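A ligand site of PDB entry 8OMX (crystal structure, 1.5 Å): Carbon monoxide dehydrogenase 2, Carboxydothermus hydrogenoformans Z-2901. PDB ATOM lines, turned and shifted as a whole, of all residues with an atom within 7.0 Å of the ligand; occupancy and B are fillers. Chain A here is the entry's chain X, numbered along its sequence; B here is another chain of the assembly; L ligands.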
ATOM      1  N   CYS A  47      34.459 -15.026  22.496  1.00  0.00           N
ATOM      2  CA  CYS A  47      34.488 -16.480  22.379  1.00  0.00           C
ATOM      3  C   CYS A  47      34.154 -17.098  23.735  1.00  0.00           C
ATOM      4  O   CYS A  47      34.593 -16.606  24.793  1.00  0.00           O
ATOM      5  CB  CYS A  47      35.841 -16.980  21.917  1.00  0.00           C
ATOM      6  SG  CYS A  47      35.866 -18.798  21.815  1.00  0.00           S
ATOM      7  N   CYS A  48      33.382 -18.176  23.706  1.00  0.00           N
ATOM      8  CA  CYS A  48      32.974 -18.865  24.932  1.00  0.00           C
ATOM      9  C   CYS A  48      33.075 -20.344  24.695  1.00  0.00           C
ATOM     10  O   CYS A  48      32.501 -20.852  23.721  1.00  0.00           O
ATOM     11  CB  CYS A  48      31.560 -18.498  25.359  1.00  0.00           C
ATOM     12  SG  CYS A  48      31.030 -19.335  26.869  1.00  0.00           S
ATOM     13  N   ARG A  49      33.759 -21.041  25.618  1.00  0.00           N
ATOM     14  CA  ARG A  49      33.846 -22.483  25.634  1.00  0.00           C
ATOM     15  C   ARG A  49      33.359 -23.016  26.983  1.00  0.00           C
ATOM     16  O   ARG A  49      33.868 -24.006  27.460  1.00  0.00           O
ATOM     17  CB  ARG A  49      35.268 -22.946  25.349  1.00  0.00           C
ATOM     18  CG  ARG A  49      35.743 -22.552  23.986  1.00  0.00           C
ATOM     19  CD  ARG A  49      37.226 -22.740  23.830  1.00  0.00           C
ATOM     20  NE  ARG A  49      37.575 -24.117  24.073  1.00  0.00           N
ATOM     21  CZ  ARG A  49      38.793 -24.540  24.388  1.00  0.00           C
ATOM     22  NH1 ARG A  49      39.803 -23.693  24.504  1.00  0.00           N
ATOM     23  NH2 ARG A  49      39.010 -25.845  24.543  1.00  0.00           N
ATOM     24  N   HIS A  50      32.400 -22.347  27.616  1.00  0.00           N
ATOM     25  CA  HIS A  50      32.020 -22.807  28.956  1.00  0.00           C
ATOM     26  C   HIS A  50      31.058 -23.981  28.941  1.00  0.00           C
ATOM     27  O   HIS A  50      30.655 -24.444  30.018  1.00  0.00           O
ATOM     28  CB  HIS A  50      31.413 -21.650  29.738  1.00  0.00           C
ATOM     29  CG  HIS A  50      32.379 -20.549  30.078  1.00  0.00           C
ATOM     30  ND1 HIS A  50      32.117 -19.623  31.052  1.00  0.00           N
ATOM     31  CD2 HIS A  50      33.606 -20.248  29.588  1.00  0.00           C
ATOM     32  CE1 HIS A  50      33.118 -18.772  31.128  1.00  0.00           C
ATOM     33  NE2 HIS A  50      34.060 -19.156  30.281  1.00  0.00           N
ATOM     34  N   CYS A  51      30.649 -24.497  27.791  1.00  0.00           N
ATOM     35  CA  CYS A  51      29.940 -25.770  27.745  1.00  0.00           C
ATOM     36  C   CYS A  51      30.233 -26.463  26.423  1.00  0.00           C
ATOM     37  O   CYS A  51      30.813 -25.881  25.514  1.00  0.00           O
ATOM     38  CB  CYS A  51      28.445 -25.578  27.972  1.00  0.00           C
ATOM     39  SG  CYS A  51      27.441 -25.123  26.522  1.00  0.00           S
ATOM     40  N   LEU A  52      29.826 -27.731  26.348  1.00  0.00           N
ATOM     41  CA  LEU A  52      30.121 -28.572  25.193  1.00  0.00           C
ATOM     42  C   LEU A  52      29.190 -28.332  24.017  1.00  0.00           C
ATOM     43  O   LEU A  52      29.291 -29.059  23.006  1.00  0.00           O
ATOM     44  CB  LEU A  52      30.075 -30.048  25.574  1.00  0.00           C
ATOM     45  CG  LEU A  52      31.014 -30.434  26.696  1.00  0.00           C
ATOM     46  CD1 LEU A  52      30.810 -31.891  27.022  1.00  0.00           C
ATOM     47  CD2 LEU A  52      32.463 -30.186  26.339  1.00  0.00           C
ATOM     48  N   GLN A  53      28.317 -27.322  24.082  1.00  0.00           N
ATOM     49  CA  GLN A  53      27.640 -26.842  22.898  1.00  0.00           C
ATOM     50  C   GLN A  53      28.530 -25.916  22.103  1.00  0.00           C
ATOM     51  O   GLN A  53      28.290 -25.706  20.908  1.00  0.00           O
ATOM     52  CB  GLN A  53      26.339 -26.136  23.260  1.00  0.00           C
ATOM     53  CG  GLN A  53      25.358 -27.141  23.813  1.00  0.00           C
ATOM     54  CD  GLN A  53      24.010 -26.614  24.197  1.00  0.00           C
ATOM     55  OE1 GLN A  53      23.024 -27.312  24.096  1.00  0.00           O
ATOM     56  NE2 GLN A  53      23.949 -25.378  24.715  1.00  0.00           N
ATOM     57  N   GLY A  54      29.549 -25.355  22.755  1.00  0.00           N
ATOM     58  CA  GLY A  54      30.464 -24.453  22.080  1.00  0.00           C
ATOM     59  C   GLY A  54      31.482 -25.208  21.240  1.00  0.00           C
ATOM     60  O   GLY A  54      31.433 -26.438  21.071  1.00  0.00           O
ATOM     61  N   PRO A  55      32.456 -24.480  20.751  1.00  0.00           N
ATOM     62  CA  PRO A  55      32.691 -23.065  21.014  1.00  0.00           C
ATOM     63  C   PRO A  55      31.686 -22.165  20.371  1.00  0.00           C
ATOM     64  O   PRO A  55      31.175 -22.361  19.248  1.00  0.00           O
ATOM     65  CB  PRO A  55      34.097 -22.809  20.415  1.00  0.00           C
ATOM     66  CG  PRO A  55      34.665 -24.132  20.119  1.00  0.00           C
ATOM     67  CD  PRO A  55      33.500 -25.065  19.898  1.00  0.00           C
ATOM     68  N   CYS A  56      31.362 -21.117  21.092  1.00  0.00           N
ATOM     69  CA  CYS A  56      30.551 -20.043  20.553  1.00  0.00           C
ATOM     70  C   CYS A  56      31.423 -18.819  20.338  1.00  0.00           C
ATOM     71  O   CYS A  56      32.247 -18.462  21.186  1.00  0.00           O
ATOM     72  CB  CYS A  56      29.401 -19.718  21.478  1.00  0.00           C
ATOM     73  SG  CYS A  56      28.192 -21.025  21.612  1.00  0.00           S
ATOM     74  N   ARG A  57      31.231 -18.186  19.206  1.00  0.00           N
ATOM     75  CA  ARG A  57      31.858 -16.907  18.968  1.00  0.00           C
ATOM     76  C   ARG A  57      30.796 -15.918  18.502  1.00  0.00           C
ATOM     77  O   ARG A  57      29.668 -16.274  18.126  1.00  0.00           O
ATOM     78  CB  ARG A  57      32.967 -17.048  17.959  1.00  0.00           C
ATOM     79  CG  ARG A  57      32.381 -17.263  16.570  1.00  0.00           C
ATOM     80  CD  ARG A  57      33.269 -17.942  15.592  1.00  0.00           C
ATOM     81  NE  ARG A  57      32.594 -18.109  14.316  1.00  0.00           N
ATOM     82  CZ  ARG A  57      31.646 -18.994  14.027  1.00  0.00           C
ATOM     83  NH1 ARG A  57      30.997 -18.964  12.871  1.00  0.00           N
ATOM     84  NH2 ARG A  57      31.332 -19.962  14.919  1.00  0.00           N
ATOM     85  N   VAL A  67      24.946 -13.974  18.941  1.00  0.00           N
ATOM     86  CA  VAL A  67      24.622 -14.371  20.299  1.00  0.00           C
ATOM     87  C   VAL A  67      25.098 -15.810  20.450  1.00  0.00           C
ATOM     88  O   VAL A  67      25.135 -16.556  19.486  1.00  0.00           O
ATOM     89  CB  VAL A  67      23.103 -14.219  20.551  1.00  0.00           C
ATOM     90  CG1 VAL A  67      22.331 -15.118  19.624  1.00  0.00           C
ATOM     91  CG2 VAL A  67      22.768 -14.497  21.940  1.00  0.00           C
ATOM     92  N   GLY A  68      25.473 -16.177  21.675  1.00  0.00           N
ATOM     93  CA  GLY A  68      25.841 -17.550  21.970  1.00  0.00           C
ATOM     94  C   GLY A  68      24.652 -18.499  21.827  1.00  0.00           C
ATOM     95  O   GLY A  68      23.503 -18.104  21.834  1.00  0.00           O
ATOM     96  N   ILE A  69      24.968 -19.772  21.767  1.00  0.00           N
ATOM     97  CA  ILE A  69      23.931 -20.751  21.486  1.00  0.00           C
ATOM     98  C   ILE A  69      22.892 -20.790  22.622  1.00  0.00           C
ATOM     99  O   ILE A  69      21.699 -20.941  22.374  1.00  0.00           O
ATOM    100  CB  ILE A  69      24.551 -22.147  21.265  1.00  0.00           C
ATOM    101  CG1 ILE A  69      25.277 -22.181  19.930  1.00  0.00           C
ATOM    102  CG2 ILE A  69      23.500 -23.257  21.403  1.00  0.00           C
ATOM    103  CD1 ILE A  69      26.049 -23.467  19.684  1.00  0.00           C
ATOM    104  N   CYS A  70      23.343 -20.651  23.877  1.00  0.00           N
ATOM    105  CA  CYS A  70      22.400 -20.646  24.990  1.00  0.00           C
ATOM    106  C   CYS A  70      21.673 -19.335  25.149  1.00  0.00           C
ATOM    107  O   CYS A  70      20.824 -19.236  26.043  1.00  0.00           O
ATOM    108  CB  CYS A  70      23.165 -20.920  26.258  1.00  0.00           C
ATOM    109  SG  CYS A  70      24.404 -19.693  26.599  1.00  0.00           S
ATOM    110  N   GLY A  71      22.029 -18.321  24.364  1.00  0.00           N
ATOM    111  CA  GLY A  71      21.455 -16.985  24.531  1.00  0.00           C
ATOM    112  C   GLY A  71      22.416 -15.979  25.123  1.00  0.00           C
ATOM    113  O   GLY A  71      22.068 -14.811  25.252  1.00  0.00           O
ATOM    114  N   ALA A  72      23.624 -16.386  25.489  1.00  0.00           N
ATOM    115  CA  ALA A  72      24.565 -15.475  26.132  1.00  0.00           C
ATOM    116  C   ALA A  72      24.954 -14.375  25.165  1.00  0.00           C
ATOM    117  O   ALA A  72      25.373 -14.624  24.031  1.00  0.00           O
ATOM    118  CB  ALA A  72      25.799 -16.243  26.565  1.00  0.00           C
ATOM    119  N   THR A  73      24.775 -13.132  25.609  1.00  0.00           N
ATOM    120  CA  THR A  73      25.116 -11.964  24.808  1.00  0.00           C
ATOM    121  C   THR A  73      26.626 -11.699  24.846  1.00  0.00           C
ATOM    122  O   THR A  73      27.374 -12.296  25.610  1.00  0.00           O
ATOM    123  CB  THR A  73      24.412 -10.731  25.332  1.00  0.00           C
ATOM    124  OG1 THR A  73      24.867 -10.531  26.674  1.00  0.00           O
ATOM    125  CG2 THR A  73      22.876 -10.833  25.308  1.00  0.00           C
ATOM    126  N   ILE A  77      29.267 -12.946  27.726  1.00  0.00           N
ATOM    127  CA  ILE A  77      30.473 -13.695  27.366  1.00  0.00           C
ATOM    128  C   ILE A  77      31.746 -12.961  27.773  1.00  0.00           C
ATOM    129  O   ILE A  77      32.629 -13.539  28.423  1.00  0.00           O
ATOM    130  CB  ILE A  77      30.472 -14.032  25.867  1.00  0.00           C
ATOM    131  CG1 ILE A  77      29.350 -15.054  25.589  1.00  0.00           C
ATOM    132  CG2 ILE A  77      31.802 -14.559  25.401  1.00  0.00           C
ATOM    133  CD1 ILE A  77      29.039 -15.374  24.110  1.00  0.00           C
ATOM    134  N   ARG A  80      32.032 -12.850  31.704  1.00  0.00           N
ATOM    135  CA  ARG A  80      32.338 -14.164  32.273  1.00  0.00           C
ATOM    136  C   ARG A  80      33.795 -14.546  32.057  1.00  0.00           C
ATOM    137  O   ARG A  80      34.470 -15.019  32.971  1.00  0.00           O
ATOM    138  CB  ARG A  80      31.412 -15.222  31.667  1.00  0.00           C
ATOM    139  CG  ARG A  80      29.974 -15.100  32.150  1.00  0.00           C
ATOM    140  CD  ARG A  80      29.131 -16.289  31.786  1.00  0.00           C
ATOM    141  NE  ARG A  80      29.205 -16.661  30.366  1.00  0.00           N
ATOM    142  CZ  ARG A  80      28.333 -17.454  29.787  1.00  0.00           C
ATOM    143  NH1 ARG A  80      27.287 -17.930  30.458  1.00  0.00           N
ATOM    144  NH2 ARG A  80      28.469 -17.764  28.506  1.00  0.00           N
ATOM    145  N   THR A 197      29.878 -18.032  36.511  1.00  0.00           N
ATOM    146  CA  THR A 197      30.260 -17.888  35.111  1.00  0.00           C
ATOM    147  C   THR A 197      30.033 -19.161  34.308  1.00  0.00           C
ATOM    148  O   THR A 197      30.228 -19.149  33.090  1.00  0.00           O
ATOM    149  CB  THR A 197      31.721 -17.442  34.984  1.00  0.00           C
ATOM    150  OG1 THR A 197      32.558 -18.427  35.614  1.00  0.00           O
ATOM    151  CG2 THR A 197      31.942 -16.070  35.605  1.00  0.00           C
ATOM    152  N   SER A 198      29.654 -20.251  34.965  1.00  0.00           N
ATOM    153  CA  SER A 198      29.348 -21.486  34.264  1.00  0.00           C
ATOM    154  C   SER A 198      28.015 -21.333  33.517  1.00  0.00           C
ATOM    155  O   SER A 198      27.275 -20.376  33.693  1.00  0.00           O
ATOM    156  CB  SER A 198      29.372 -22.675  35.247  1.00  0.00           C
ATOM    157  OG  SER A 198      28.223 -22.703  36.068  1.00  0.00           O
ATOM    158  N   MET A 199      27.752 -22.279  32.604  1.00  0.00           N
ATOM    159  CA  MET A 199      26.623 -22.147  31.681  1.00  0.00           C
ATOM    160  C   MET A 199      25.309 -22.014  32.451  1.00  0.00           C
ATOM    161  O   MET A 199      25.034 -22.760  33.406  1.00  0.00           O
ATOM    162  CB  MET A 199      26.579 -23.339  30.712  1.00  0.00           C
ATOM    163  CG  MET A 199      25.462 -23.337  29.657  1.00  0.00           C
ATOM    164  SD  MET A 199      23.894 -23.911  30.361  1.00  0.00           S
ATOM    165  CE  MET A 199      22.802 -23.729  28.993  1.00  0.00           C
ATOM    166  N   GLY A 200      24.472 -21.088  31.997  1.00  0.00           N
ATOM    167  CA  GLY A 200      23.125 -20.947  32.516  1.00  0.00           C
ATOM    168  C   GLY A 200      23.028 -20.400  33.911  1.00  0.00           C
ATOM    169  O   GLY A 200      22.066 -20.707  34.632  1.00  0.00           O
ATOM    170  N   VAL B  28      17.182 -22.065  20.598  1.00  0.00           N
ATOM    171  CA  VAL B  28      18.524 -22.606  20.765  1.00  0.00           C
ATOM    172  C   VAL B  28      18.985 -23.318  19.488  1.00  0.00           C
ATOM    173  O   VAL B  28      20.177 -23.247  19.115  1.00  0.00           O
ATOM    174  CB  VAL B  28      18.526 -23.534  21.994  1.00  0.00           C
ATOM    175  CG1 VAL B  28      17.568 -24.729  21.786  1.00  0.00           C
ATOM    176  CG2 VAL B  28      19.913 -23.991  22.301  1.00  0.00           C
ATOM    177  N   MET B  35      25.708 -20.540  14.342  1.00  0.00           N
ATOM    178  CA  MET B  35      27.078 -20.692  14.839  1.00  0.00           C
ATOM    179  C   MET B  35      27.922 -21.599  13.958  1.00  0.00           C
ATOM    180  O   MET B  35      29.148 -21.646  14.138  1.00  0.00           O
ATOM    181  CB  MET B  35      27.028 -21.251  16.262  1.00  0.00           C
ATOM    182  CG  MET B  35      28.266 -20.988  17.074  1.00  0.00           C
ATOM    183  SD  MET B  35      28.684 -19.240  17.276  1.00  0.00           S
ATOM    184  CE  MET B  35      27.402 -18.657  18.361  1.00  0.00           C
ATOM    185  N   GLN B  38      31.426 -24.346  13.560  1.00  0.00           N
ATOM    186  CA  GLN B  38      32.062 -23.951  14.806  1.00  0.00           C
ATOM    187  C   GLN B  38      33.569 -24.086  14.706  1.00  0.00           C
ATOM    188  O   GLN B  38      34.108 -24.798  13.864  1.00  0.00           O
ATOM    189  CB  GLN B  38      31.491 -24.789  15.953  1.00  0.00           C
ATOM    190  CG  GLN B  38      30.060 -24.427  16.248  1.00  0.00           C
ATOM    191  CD  GLN B  38      29.453 -25.240  17.375  1.00  0.00           C
ATOM    192  OE1 GLN B  38      29.039 -26.396  17.190  1.00  0.00           O
ATOM    193  NE2 GLN B  38      29.415 -24.648  18.566  1.00  0.00           N
ATOM    194  N   PRO B 336      19.925 -18.105  29.004  1.00  0.00           N
ATOM    195  CA  PRO B 336      19.555 -16.705  29.265  1.00  0.00           C
ATOM    196  C   PRO B 336      18.600 -16.145  28.239  1.00  0.00           C
ATOM    197  O   PRO B 336      17.965 -15.114  28.485  1.00  0.00           O
ATOM    198  CB  PRO B 336      20.899 -15.969  29.272  1.00  0.00           C
ATOM    199  CG  PRO B 336      21.857 -16.886  28.595  1.00  0.00           C
ATOM    200  CD  PRO B 336      21.388 -18.278  28.919  1.00  0.00           C
ATOM    201  N   MET B 560      26.539 -31.675  28.218  1.00  0.00           N
ATOM    202  CA  MET B 560      26.678 -30.279  27.843  1.00  0.00           C
ATOM    203  C   MET B 560      27.485 -29.506  28.890  1.00  0.00           C
ATOM    204  O   MET B 560      28.468 -28.854  28.545  1.00  0.00           O
ATOM    205  CB  MET B 560      25.303 -29.656  27.683  1.00  0.00           C
ATOM    206  CG  MET B 560      25.286 -28.214  27.297  1.00  0.00           C
ATOM    207  SD  MET B 560      25.106 -27.129  28.741  1.00  0.00           S
ATOM    208  CE  MET B 560      23.522 -27.564  29.377  1.00  0.00           C
HETATM  209 FE1  LIG L   1      28.012 -21.309  23.950  1.00  0.00          FE
HETATM  210 FE2  LIG L   1      27.917 -22.914  26.096  1.00  0.00          FE
HETATM  211 FE3  LIG L   1      29.158 -20.561  26.163  1.00  0.00          FE
HETATM  212 FE4  LIG L   1      26.437 -20.570  26.075  1.00  0.00          FE
HETATM  213  S1  LIG L   1      27.814 -21.383  27.746  1.00  0.00           S
HETATM  214  S2  LIG L   1      27.848 -19.221  24.917  1.00  0.00           S
HETATM  215  S3  LIG L   1      26.226 -22.375  24.720  1.00  0.00           S
HETATM  216  S4  LIG L   1      29.691 -22.314  24.940  1.00  0.00           S
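The backbone NH (N) of Cys 70 lies close to a sulfur (S3) of the ligand, at 3.5 Å.
FE4 of the ligand is bound by SG of Cys 70 (2.3 Å).
S4 of the ligand lies close to N of Cys 51 (3.7 Å).
An iron atom (FE2) of the ligand is bound by the side-chain sulfur of Cys 51, at 2.3 Å.
FE3 of the ligand is bound by SG of Cys 48 (2.3 Å).
An iron atom (FE1) of the ligand is bound by the side-chain sulfur (SG) of Cys 56, at 2.4 Å.
The backbone NH (N) of Gly 54 lies close to a sulfur (S4) of the ligand, at 3.7 Å.
The guanidinium group of Arg 80 lies close to a sulfur (S1) of the ligand, 3.8 Å away.
The side-chain amide nitrogen (NE2) of Gln 53 sits close to a sulfur (S3) of the ligand (3.8 Å).
The side-chain sulfur of Cys 70 sits close to the backbone NH of Ala 72 (3.6 Å).
The side-chain sulfur (SG) of Cys 51 sits close to the backbone NH (N) of Gln 53.
The side-chain sulfur (SG) of Cys 51 sits close to the side-chain sulfur (SD) of Met 560 of chain B, at 3.8 Å.
The guanidinium group (NH2) of Arg 80 lies close to the side-chain sulfur (SG) of Cys 48.
The side-chain sulfur (SG) of Cys 48 sits close to the backbone NH (N) of His 50, 3.4 Å away.
The side-chain sulfur (SG) of Cys 47 sits close to the backbone carbonyl oxygen (O) of Cys 56.
NE2 of Gln 38 of chain B is in hydrogen-bond range of O of Gln 53 (2.8 Å).
The backbone carbonyl oxygen (O) of Thr 197 sits at hydrogen-bond distance from a ring nitrogen (ND1) of His 50 (2.8 Å).
His 50 touches the ligand (N to S4, 3.8 Å).
Gly 68 touches the ligand.
Ile 69 touches the ligand (CB to S3, 3.8 Å).
CB of Ala 72 touches S2 of the ligand, at 3.97 Å.
CG of Met 199 touches S1 of the ligand, at 3.6 Å.
Hydrophobic or aromatic side chains that line the ligand: Ile 69, Ala 72 and Met 199.
Of the 29 residues printed, 12 come within 4 Å of the ligand.
The nearest printed residue that does not touch the ligand is Ile 77 (4.1 Å).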
